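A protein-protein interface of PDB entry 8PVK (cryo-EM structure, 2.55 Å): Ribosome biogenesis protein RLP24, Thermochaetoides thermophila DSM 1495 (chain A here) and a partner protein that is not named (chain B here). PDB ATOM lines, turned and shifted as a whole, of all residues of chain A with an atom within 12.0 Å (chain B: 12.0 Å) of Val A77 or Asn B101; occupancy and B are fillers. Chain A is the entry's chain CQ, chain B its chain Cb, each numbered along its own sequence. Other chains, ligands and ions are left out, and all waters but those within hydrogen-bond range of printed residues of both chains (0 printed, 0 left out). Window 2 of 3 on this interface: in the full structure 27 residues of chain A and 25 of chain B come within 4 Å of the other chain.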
ATOM      1  N   ARG A   2     -12.095  -9.808 -20.534  1.00  0.00           N
ATOM      2  CA  ARG A   2     -13.515  -9.895 -20.226  1.00  0.00           C
ATOM      3  C   ARG A   2     -13.762  -9.278 -18.857  1.00  0.00           C
ATOM      4  O   ARG A   2     -12.841  -8.805 -18.188  1.00  0.00           O
ATOM      5  CB  ARG A   2     -14.009 -11.345 -20.269  1.00  0.00           C
ATOM      6  CG  ARG A   2     -13.467 -12.218 -19.153  1.00  0.00           C
ATOM      7  CD  ARG A   2     -14.032 -13.623 -19.228  1.00  0.00           C
ATOM      8  NE  ARG A   2     -15.409 -13.684 -18.753  1.00  0.00           N
ATOM      9  CZ  ARG A   2     -16.467 -13.826 -19.539  1.00  0.00           C
ATOM     10  NH1 ARG A   2     -16.345 -13.921 -20.853  1.00  0.00           N
ATOM     11  NH2 ARG A   2     -17.679 -13.873 -18.993  1.00  0.00           N
ATOM     12  N   GLN A  70     -32.031 -13.768 -20.097  1.00  0.00           N
ATOM     13  CA  GLN A  70     -31.666 -15.059 -20.661  1.00  0.00           C
ATOM     14  C   GLN A  70     -30.722 -14.937 -21.851  1.00  0.00           C
ATOM     15  O   GLN A  70     -30.423 -15.948 -22.494  1.00  0.00           O
ATOM     16  CB  GLN A  70     -32.926 -15.823 -21.077  1.00  0.00           C
ATOM     17  CG  GLN A  70     -33.733 -16.365 -19.912  1.00  0.00           C
ATOM     18  CD  GLN A  70     -33.080 -17.569 -19.260  1.00  0.00           C
ATOM     19  OE1 GLN A  70     -32.442 -18.382 -19.929  1.00  0.00           O
ATOM     20  NE2 GLN A  70     -33.237 -17.686 -17.946  1.00  0.00           N
ATOM     21  N   PHE A  71     -30.249 -13.731 -22.157  1.00  0.00           N
ATOM     22  CA  PHE A  71     -29.392 -13.521 -23.315  1.00  0.00           C
ATOM     23  C   PHE A  71     -27.907 -13.599 -22.992  1.00  0.00           C
ATOM     24  O   PHE A  71     -27.106 -13.861 -23.896  1.00  0.00           O
ATOM     25  CB  PHE A  71     -29.696 -12.162 -23.951  1.00  0.00           C
ATOM     26  CG  PHE A  71     -31.017 -12.109 -24.658  1.00  0.00           C
ATOM     27  CD1 PHE A  71     -31.127 -12.507 -25.979  1.00  0.00           C
ATOM     28  CD2 PHE A  71     -32.150 -11.655 -24.002  1.00  0.00           C
ATOM     29  CE1 PHE A  71     -32.342 -12.456 -26.632  1.00  0.00           C
ATOM     30  CE2 PHE A  71     -33.368 -11.602 -24.650  1.00  0.00           C
ATOM     31  CZ  PHE A  71     -33.463 -12.004 -25.966  1.00  0.00           C
ATOM     32  N   ALA A  72     -27.521 -13.380 -21.739  1.00  0.00           N
ATOM     33  CA  ALA A  72     -26.123 -13.396 -21.336  1.00  0.00           C
ATOM     34  C   ALA A  72     -25.808 -14.708 -20.632  1.00  0.00           C
ATOM     35  O   ALA A  72     -26.480 -15.074 -19.661  1.00  0.00           O
ATOM     36  CB  ALA A  72     -25.806 -12.212 -20.421  1.00  0.00           C
ATOM     37  N   ALA A  73     -24.790 -15.410 -21.122  1.00  0.00           N
ATOM     38  CA  ALA A  73     -24.403 -16.691 -20.555  1.00  0.00           C
ATOM     39  C   ALA A  73     -22.939 -16.958 -20.864  1.00  0.00           C
ATOM     40  O   ALA A  73     -22.350 -16.353 -21.761  1.00  0.00           O
ATOM     41  CB  ALA A  73     -25.275 -17.832 -21.090  1.00  0.00           C
ATOM     42  N   ARG A  74     -22.355 -17.880 -20.101  1.00  0.00           N
ATOM     43  CA  ARG A  74     -21.001 -18.352 -20.357  1.00  0.00           C
ATOM     44  C   ARG A  74     -21.057 -19.366 -21.493  1.00  0.00           C
ATOM     45  O   ARG A  74     -21.525 -20.492 -21.305  1.00  0.00           O
ATOM     46  CB  ARG A  74     -20.402 -18.962 -19.093  1.00  0.00           C
ATOM     47  CG  ARG A  74     -18.994 -19.513 -19.258  1.00  0.00           C
ATOM     48  CD  ARG A  74     -18.366 -19.796 -17.902  1.00  0.00           C
ATOM     49  NE  ARG A  74     -17.175 -20.631 -17.995  1.00  0.00           N
ATOM     50  CZ  ARG A  74     -15.955 -20.176 -18.244  1.00  0.00           C
ATOM     51  NH1 ARG A  74     -15.725 -18.889 -18.445  1.00  0.00           N
ATOM     52  NH2 ARG A  74     -14.939 -21.033 -18.292  1.00  0.00           N
ATOM     53  N   ARG A  75     -20.586 -18.967 -22.670  1.00  0.00           N
ATOM     54  CA  ARG A  75     -20.691 -19.792 -23.870  1.00  0.00           C
ATOM     55  C   ARG A  75     -19.499 -20.740 -23.922  1.00  0.00           C
ATOM     56  O   ARG A  75     -18.379 -20.325 -24.238  1.00  0.00           O
ATOM     57  CB  ARG A  75     -20.756 -18.919 -25.119  1.00  0.00           C
ATOM     58  CG  ARG A  75     -21.739 -17.770 -25.014  1.00  0.00           C
ATOM     59  CD  ARG A  75     -23.166 -18.231 -25.234  1.00  0.00           C
ATOM     60  NE  ARG A  75     -24.122 -17.164 -24.965  1.00  0.00           N
ATOM     61  CZ  ARG A  75     -25.418 -17.232 -25.228  1.00  0.00           C
ATOM     62  NH1 ARG A  75     -25.956 -18.309 -25.777  1.00  0.00           N
ATOM     63  NH2 ARG A  75     -26.195 -16.194 -24.935  1.00  0.00           N
ATOM     64  N   ASN A  76     -19.742 -22.010 -23.614  1.00  0.00           N
ATOM     65  CA  ASN A  76     -18.697 -23.022 -23.640  1.00  0.00           C
ATOM     66  C   ASN A  76     -18.500 -23.640 -25.017  1.00  0.00           C
ATOM     67  O   ASN A  76     -17.527 -24.376 -25.213  1.00  0.00           O
ATOM     68  CB  ASN A  76     -19.011 -24.125 -22.626  1.00  0.00           C
ATOM     69  CG  ASN A  76     -18.683 -23.718 -21.206  1.00  0.00           C
ATOM     70  OD1 ASN A  76     -17.971 -22.742 -20.976  1.00  0.00           O
ATOM     71  ND2 ASN A  76     -19.194 -24.472 -20.241  1.00  0.00           N
ATOM     72  N   VAL A  77     -19.388 -23.363 -25.964  1.00  0.00           N
ATOM     73  CA  VAL A  77     -19.275 -23.838 -27.337  1.00  0.00           C
ATOM     74  C   VAL A  77     -18.974 -22.628 -28.219  1.00  0.00           C
ATOM     75  O   VAL A  77     -19.860 -21.788 -28.436  1.00  0.00           O
ATOM     76  CB  VAL A  77     -20.548 -24.561 -27.794  1.00  0.00           C
ATOM     77  CG1 VAL A  77     -20.359 -25.140 -29.184  1.00  0.00           C
ATOM     78  CG2 VAL A  77     -20.914 -25.655 -26.806  1.00  0.00           C
ATOM     79  N   PRO A  78     -17.750 -22.485 -28.725  1.00  0.00           N
ATOM     80  CA  PRO A  78     -17.412 -21.305 -29.529  1.00  0.00           C
ATOM     81  C   PRO A  78     -18.109 -21.300 -30.879  1.00  0.00           C
ATOM     82  O   PRO A  78     -18.460 -22.344 -31.436  1.00  0.00           O
ATOM     83  CB  PRO A  78     -15.893 -21.414 -29.695  1.00  0.00           C
ATOM     84  CG  PRO A  78     -15.603 -22.865 -29.526  1.00  0.00           C
ATOM     85  CD  PRO A  78     -16.584 -23.357 -28.509  1.00  0.00           C
ATOM     86  N   VAL A  79     -18.302 -20.094 -31.402  1.00  0.00           N
ATOM     87  CA  VAL A  79     -18.921 -19.868 -32.701  1.00  0.00           C
ATOM     88  C   VAL A  79     -17.876 -19.246 -33.617  1.00  0.00           C
ATOM     89  O   VAL A  79     -17.099 -18.387 -33.186  1.00  0.00           O
ATOM     90  CB  VAL A  79     -20.166 -18.962 -32.581  1.00  0.00           C
ATOM     91  CG1 VAL A  79     -20.887 -18.838 -33.915  1.00  0.00           C
ATOM     92  CG2 VAL A  79     -21.108 -19.496 -31.515  1.00  0.00           C
ATOM     93  N   ARG A  80     -17.836 -19.711 -34.867  1.00  0.00           N
ATOM     94  CA  ARG A  80     -16.937 -19.140 -35.862  1.00  0.00           C
ATOM     95  C   ARG A  80     -17.265 -17.669 -36.089  1.00  0.00           C
ATOM     96  O   ARG A  80     -18.433 -17.272 -36.089  1.00  0.00           O
ATOM     97  CB  ARG A  80     -17.045 -19.921 -37.172  1.00  0.00           C
ATOM     98  CG  ARG A  80     -15.986 -19.579 -38.205  1.00  0.00           C
ATOM     99  CD  ARG A  80     -15.994 -20.580 -39.347  1.00  0.00           C
ATOM    100  NE  ARG A  80     -15.746 -21.940 -38.887  1.00  0.00           N
ATOM    101  CZ  ARG A  80     -14.539 -22.470 -38.731  1.00  0.00           C
ATOM    102  NH1 ARG A  80     -13.442 -21.777 -38.987  1.00  0.00           N
ATOM    103  NH2 ARG A  80     -14.432 -23.725 -38.306  1.00  0.00           N
ATOM    104  N   TYR A  81     -16.222 -16.857 -36.265  1.00  0.00           N
ATOM    105  CA  TYR A  81     -16.389 -15.410 -36.283  1.00  0.00           C
ATOM    106  C   TYR A  81     -17.127 -14.958 -37.539  1.00  0.00           C
ATOM    107  O   TYR A  81     -16.828 -15.411 -38.648  1.00  0.00           O
ATOM    108  CB  TYR A  81     -15.033 -14.713 -36.187  1.00  0.00           C
ATOM    109  CG  TYR A  81     -15.091 -13.241 -36.522  1.00  0.00           C
ATOM    110  CD1 TYR A  81     -15.700 -12.342 -35.656  1.00  0.00           C
ATOM    111  CD2 TYR A  81     -14.535 -12.748 -37.695  1.00  0.00           C
ATOM    112  CE1 TYR A  81     -15.763 -10.997 -35.952  1.00  0.00           C
ATOM    113  CE2 TYR A  81     -14.591 -11.403 -37.999  1.00  0.00           C
ATOM    114  CZ  TYR A  81     -15.205 -10.533 -37.123  1.00  0.00           C
ATOM    115  OH  TYR A  81     -15.265  -9.192 -37.420  1.00  0.00           O
ATOM    116  N   ASN A  82     -18.091 -14.057 -37.355  1.00  0.00           N
ATOM    117  CA  ASN A  82     -18.900 -13.530 -38.447  1.00  0.00           C
ATOM    118  C   ASN A  82     -19.192 -12.066 -38.150  1.00  0.00           C
ATOM    119  O   ASN A  82     -19.809 -11.752 -37.125  1.00  0.00           O
ATOM    120  CB  ASN A  82     -20.196 -14.334 -38.605  1.00  0.00           C
ATOM    121  CG  ASN A  82     -20.870 -14.113 -39.947  1.00  0.00           C
ATOM    122  OD1 ASN A  82     -21.074 -12.981 -40.381  1.00  0.00           O
ATOM    123  ND2 ASN A  82     -21.213 -15.207 -40.617  1.00  0.00           N
ATOM    124  N   LEU A  85     -22.758 -11.055 -37.643  1.00  0.00           N
ATOM    125  CA  LEU A  85     -23.254 -11.613 -36.390  1.00  0.00           C
ATOM    126  C   LEU A  85     -22.823 -10.765 -35.201  1.00  0.00           C
ATOM    127  O   LEU A  85     -23.636 -10.469 -34.320  1.00  0.00           O
ATOM    128  CB  LEU A  85     -22.769 -13.053 -36.229  1.00  0.00           C
ATOM    129  CG  LEU A  85     -23.133 -13.751 -34.917  1.00  0.00           C
ATOM    130  CD1 LEU A  85     -24.638 -13.904 -34.797  1.00  0.00           C
ATOM    131  CD2 LEU A  85     -22.449 -15.102 -34.825  1.00  0.00           C
ATOM    132  N   TRP A  86     -21.557 -10.337 -35.174  1.00  0.00           N
ATOM    133  CA  TRP A  86     -21.091  -9.459 -34.098  1.00  0.00           C
ATOM    134  C   TRP A  86     -21.773  -8.089 -34.115  1.00  0.00           C
ATOM    135  O   TRP A  86     -22.117  -7.559 -33.049  1.00  0.00           O
ATOM    136  CB  TRP A  86     -19.566  -9.333 -34.148  1.00  0.00           C
ATOM    137  CG  TRP A  86     -18.842 -10.282 -33.213  1.00  0.00           C
ATOM    138  CD1 TRP A  86     -18.248  -9.949 -32.029  1.00  0.00           C
ATOM    139  CD2 TRP A  86     -18.718 -11.708 -33.327  1.00  0.00           C
ATOM    140  NE1 TRP A  86     -17.718 -11.062 -31.430  1.00  0.00           N
ATOM    141  CE2 TRP A  86     -17.997 -12.156 -32.202  1.00  0.00           C
ATOM    142  CE3 TRP A  86     -19.130 -12.644 -34.276  1.00  0.00           C
ATOM    143  CZ2 TRP A  86     -17.681 -13.498 -32.004  1.00  0.00           C
ATOM    144  CZ3 TRP A  86     -18.814 -13.974 -34.079  1.00  0.00           C
ATOM    145  CH2 TRP A  86     -18.096 -14.389 -32.953  1.00  0.00           C
ATOM    146  N   GLU B  89     -22.606 -21.471  -7.884  1.00  0.00           N
ATOM    147  CA  GLU B  89     -23.908 -21.546  -8.542  1.00  0.00           C
ATOM    148  C   GLU B  89     -24.860 -20.486  -8.001  1.00  0.00           C
ATOM    149  O   GLU B  89     -25.548 -19.803  -8.769  1.00  0.00           O
ATOM    150  CB  GLU B  89     -24.504 -22.947  -8.376  1.00  0.00           C
ATOM    151  CG  GLU B  89     -23.755 -24.059  -9.108  1.00  0.00           C
ATOM    152  CD  GLU B  89     -22.551 -24.586  -8.349  1.00  0.00           C
ATOM    153  OE1 GLU B  89     -22.313 -24.137  -7.208  1.00  0.00           O
ATOM    154  OE2 GLU B  89     -21.841 -25.455  -8.897  1.00  0.00           O
ATOM    155  N   MET B  92     -23.725 -17.096  -9.310  1.00  0.00           N
ATOM    156  CA  MET B  92     -24.211 -16.822 -10.661  1.00  0.00           C
ATOM    157  C   MET B  92     -25.706 -16.523 -10.668  1.00  0.00           C
ATOM    158  O   MET B  92     -26.164 -15.634 -11.399  1.00  0.00           O
ATOM    159  CB  MET B  92     -23.904 -17.993 -11.593  1.00  0.00           C
ATOM    160  CG  MET B  92     -22.431 -18.223 -11.857  1.00  0.00           C
ATOM    161  SD  MET B  92     -22.160 -19.577 -13.014  1.00  0.00           S
ATOM    162  CE  MET B  92     -22.526 -20.987 -11.976  1.00  0.00           C
ATOM    163  N   TYR B  97     -26.723 -15.147 -14.074  1.00  0.00           N
ATOM    164  CA  TYR B  97     -25.742 -15.680 -15.004  1.00  0.00           C
ATOM    165  C   TYR B  97     -25.896 -17.193 -15.081  1.00  0.00           C
ATOM    166  O   TYR B  97     -26.142 -17.851 -14.066  1.00  0.00           O
ATOM    167  CB  TYR B  97     -24.326 -15.310 -14.558  1.00  0.00           C
ATOM    168  CG  TYR B  97     -23.279 -15.388 -15.642  1.00  0.00           C
ATOM    169  CD1 TYR B  97     -23.377 -14.609 -16.788  1.00  0.00           C
ATOM    170  CD2 TYR B  97     -22.180 -16.226 -15.510  1.00  0.00           C
ATOM    171  CE1 TYR B  97     -22.416 -14.672 -17.778  1.00  0.00           C
ATOM    172  CE2 TYR B  97     -21.213 -16.296 -16.493  1.00  0.00           C
ATOM    173  CZ  TYR B  97     -21.336 -15.517 -17.625  1.00  0.00           C
ATOM    174  OH  TYR B  97     -20.375 -15.582 -18.605  1.00  0.00           O
ATOM    175  N   ARG B  98     -25.757 -17.740 -16.285  1.00  0.00           N
ATOM    176  CA  ARG B  98     -25.912 -19.170 -16.498  1.00  0.00           C
ATOM    177  C   ARG B  98     -24.798 -19.667 -17.406  1.00  0.00           C
ATOM    178  O   ARG B  98     -24.088 -18.885 -18.045  1.00  0.00           O
ATOM    179  CB  ARG B  98     -27.283 -19.507 -17.098  1.00  0.00           C
ATOM    180  CG  ARG B  98     -27.694 -18.610 -18.249  1.00  0.00           C
ATOM    181  CD  ARG B  98     -28.818 -19.234 -19.052  1.00  0.00           C
ATOM    182  NE  ARG B  98     -29.011 -18.568 -20.335  1.00  0.00           N
ATOM    183  CZ  ARG B  98     -28.878 -19.161 -21.513  1.00  0.00           C
ATOM    184  NH1 ARG B  98     -28.544 -20.437 -21.611  1.00  0.00           N
ATOM    185  NH2 ARG B  98     -29.085 -18.456 -22.621  1.00  0.00           N
ATOM    186  N   ILE B  99     -24.651 -20.987 -17.457  1.00  0.00           N
ATOM    187  CA  ILE B  99     -23.660 -21.649 -18.296  1.00  0.00           C
ATOM    188  C   ILE B  99     -24.386 -22.315 -19.453  1.00  0.00           C
ATOM    189  O   ILE B  99     -25.337 -23.078 -19.242  1.00  0.00           O
ATOM    190  CB  ILE B  99     -22.838 -22.675 -17.496  1.00  0.00           C
ATOM    191  CG1 ILE B  99     -22.093 -21.987 -16.351  1.00  0.00           C
ATOM    192  CG2 ILE B  99     -21.863 -23.404 -18.401  1.00  0.00           C
ATOM    193  CD1 ILE B  99     -21.865 -22.883 -15.157  1.00  0.00           C
ATOM    194  N   ASP B 100     -23.942 -22.028 -20.672  1.00  0.00           N
ATOM    195  CA  ASP B 100     -24.530 -22.583 -21.885  1.00  0.00           C
ATOM    196  C   ASP B 100     -23.562 -23.633 -22.415  1.00  0.00           C
ATOM    197  O   ASP B 100     -22.519 -23.293 -22.986  1.00  0.00           O
ATOM    198  CB  ASP B 100     -24.790 -21.480 -22.912  1.00  0.00           C
ATOM    199  CG  ASP B 100     -25.367 -22.004 -24.222  1.00  0.00           C
ATOM    200  OD1 ASP B 100     -25.378 -21.232 -25.203  1.00  0.00           O
ATOM    201  OD2 ASP B 100     -25.852 -23.154 -24.271  1.00  0.00           O
ATOM    202  N   ASN B 101     -23.909 -24.905 -22.230  1.00  0.00           N
ATOM    203  CA  ASN B 101     -23.091 -26.018 -22.689  1.00  0.00           C
ATOM    204  C   ASN B 101     -23.615 -26.639 -23.976  1.00  0.00           C
ATOM    205  O   ASN B 101     -23.156 -27.718 -24.362  1.00  0.00           O
ATOM    206  CB  ASN B 101     -22.996 -27.086 -21.598  1.00  0.00           C
ATOM    207  CG  ASN B 101     -22.191 -26.625 -20.402  1.00  0.00           C
ATOM    208  OD1 ASN B 101     -21.113 -26.054 -20.549  1.00  0.00           O
ATOM    209  ND2 ASN B 101     -22.712 -26.874 -19.207  1.00  0.00           N
ATOM    210  N   GLY B 102     -24.561 -25.988 -24.644  1.00  0.00           N
ATOM    211  CA  GLY B 102     -25.124 -26.516 -25.873  1.00  0.00           C
ATOM    212  C   GLY B 102     -26.463 -27.197 -25.670  1.00  0.00           C
ATOM    213  O   GLY B 102     -27.170 -27.496 -26.633  1.00  0.00           O
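Of chain B, only Asn B101 comes within 4 Å of Val A77.
Asn B101 touches just these residues of chain A: Asn A76 and Val A77.
Of chain B, only Ile B99 (3.4 Å), Asp B100 (3.1 Å) and Asn B101 (2.5 Å) come within 4 Å of Asn A76.
No residue of chain B comes within 4 Å of Pro A78.
No residue of chain B comes within 4 Å of Val A79.
Of chain A, only Arg A74 and Asn A76 come within 4 Å of Ile B99.
Of chain A, only Arg A74 (2.9 Å), Arg A75 (3.0 Å) and Asn A76 (3.1 Å) come within 4 Å of Asp B100.
Gly B102 touches none of the printed residues of chain A.
Printed residues of chain B within 4 Å of Arg A2: Tyr B97.
Of the printed residues of chain A, Arg B98 touches Gln A70 (2.8 Å), Ala A72 (3.996 Å), Ala A73 (3.3 Å) and Arg A74 (2.9 Å).
Asn A82 touches none of the printed residues of chain B.
The nearest residue of chain B that does not touch Val A77 is Gly B102 (4.3 Å).
The nearest printed residue of chain B that does not touch Ala A73 is Asp B100 (4.1 Å).
Of the 16 printed residues of chain A, 8 touch a printed residue of chain B.
Printed residues of chain A that touch a printed residue of chain B: Arg A2, Gln A70, Ala A72, Ala A73, Arg A74, Arg A75, Asn A76 and Val A77.
Hydrophobic or aromatic side chains of chain B that line the printed part of chain A: Tyr B97 and Ile B99.
Among the printed residues, pairs that only touch across the chains: Ala A72 with Arg B98, Ala A73 with Tyr B97, Ala A73 with Arg B98, Arg A74 with Ile B99, Asn A76 with Ile B99 and Val A77 with Asn B101.
NH2 of Arg B98 sits at hydrogen-bond distance from O of Gln A70.
OD1 of Asp B100 is in salt-bridge range of NH1 of Arg A75 (3.0 Å).
The side-chain hydroxyl (OH) of Tyr B97 lies within hydrogen-bond range of the guanidinium group (NH2) of Arg A2 (3.2 Å).
The backbone carbonyl oxygen (O) of Arg A74 is in hydrogen-bond range of the backbone NH (N) of Asp B100 (2.9 Å).
The backbone carbonyl oxygen (O) of Arg B98 lies within hydrogen-bond range of the backbone NH (N) of Arg A74.
The backbone NH (N) of Asn A76 is in hydrogen-bond range of the backbone carbonyl oxygen (O) of Asp B100 (3.1 Å).
OD1 of Asn B101 is in hydrogen-bond range of ND2 of Asn A76.
OH of Tyr B97 sits close to N of Arg A74.
The side-chain carboxylate of Asp B100 sits at hydrogen-bond distance from the backbone NH of Gly B102, 3.1 Å away.
The backbone NH of Tyr B97 sits at hydrogen-bond distance from the backbone carbonyl oxygen of Met B92 (2.8 Å).
NH2 of Arg A75 is in hydrogen-bond range of O of Phe A71 (2.7 Å).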
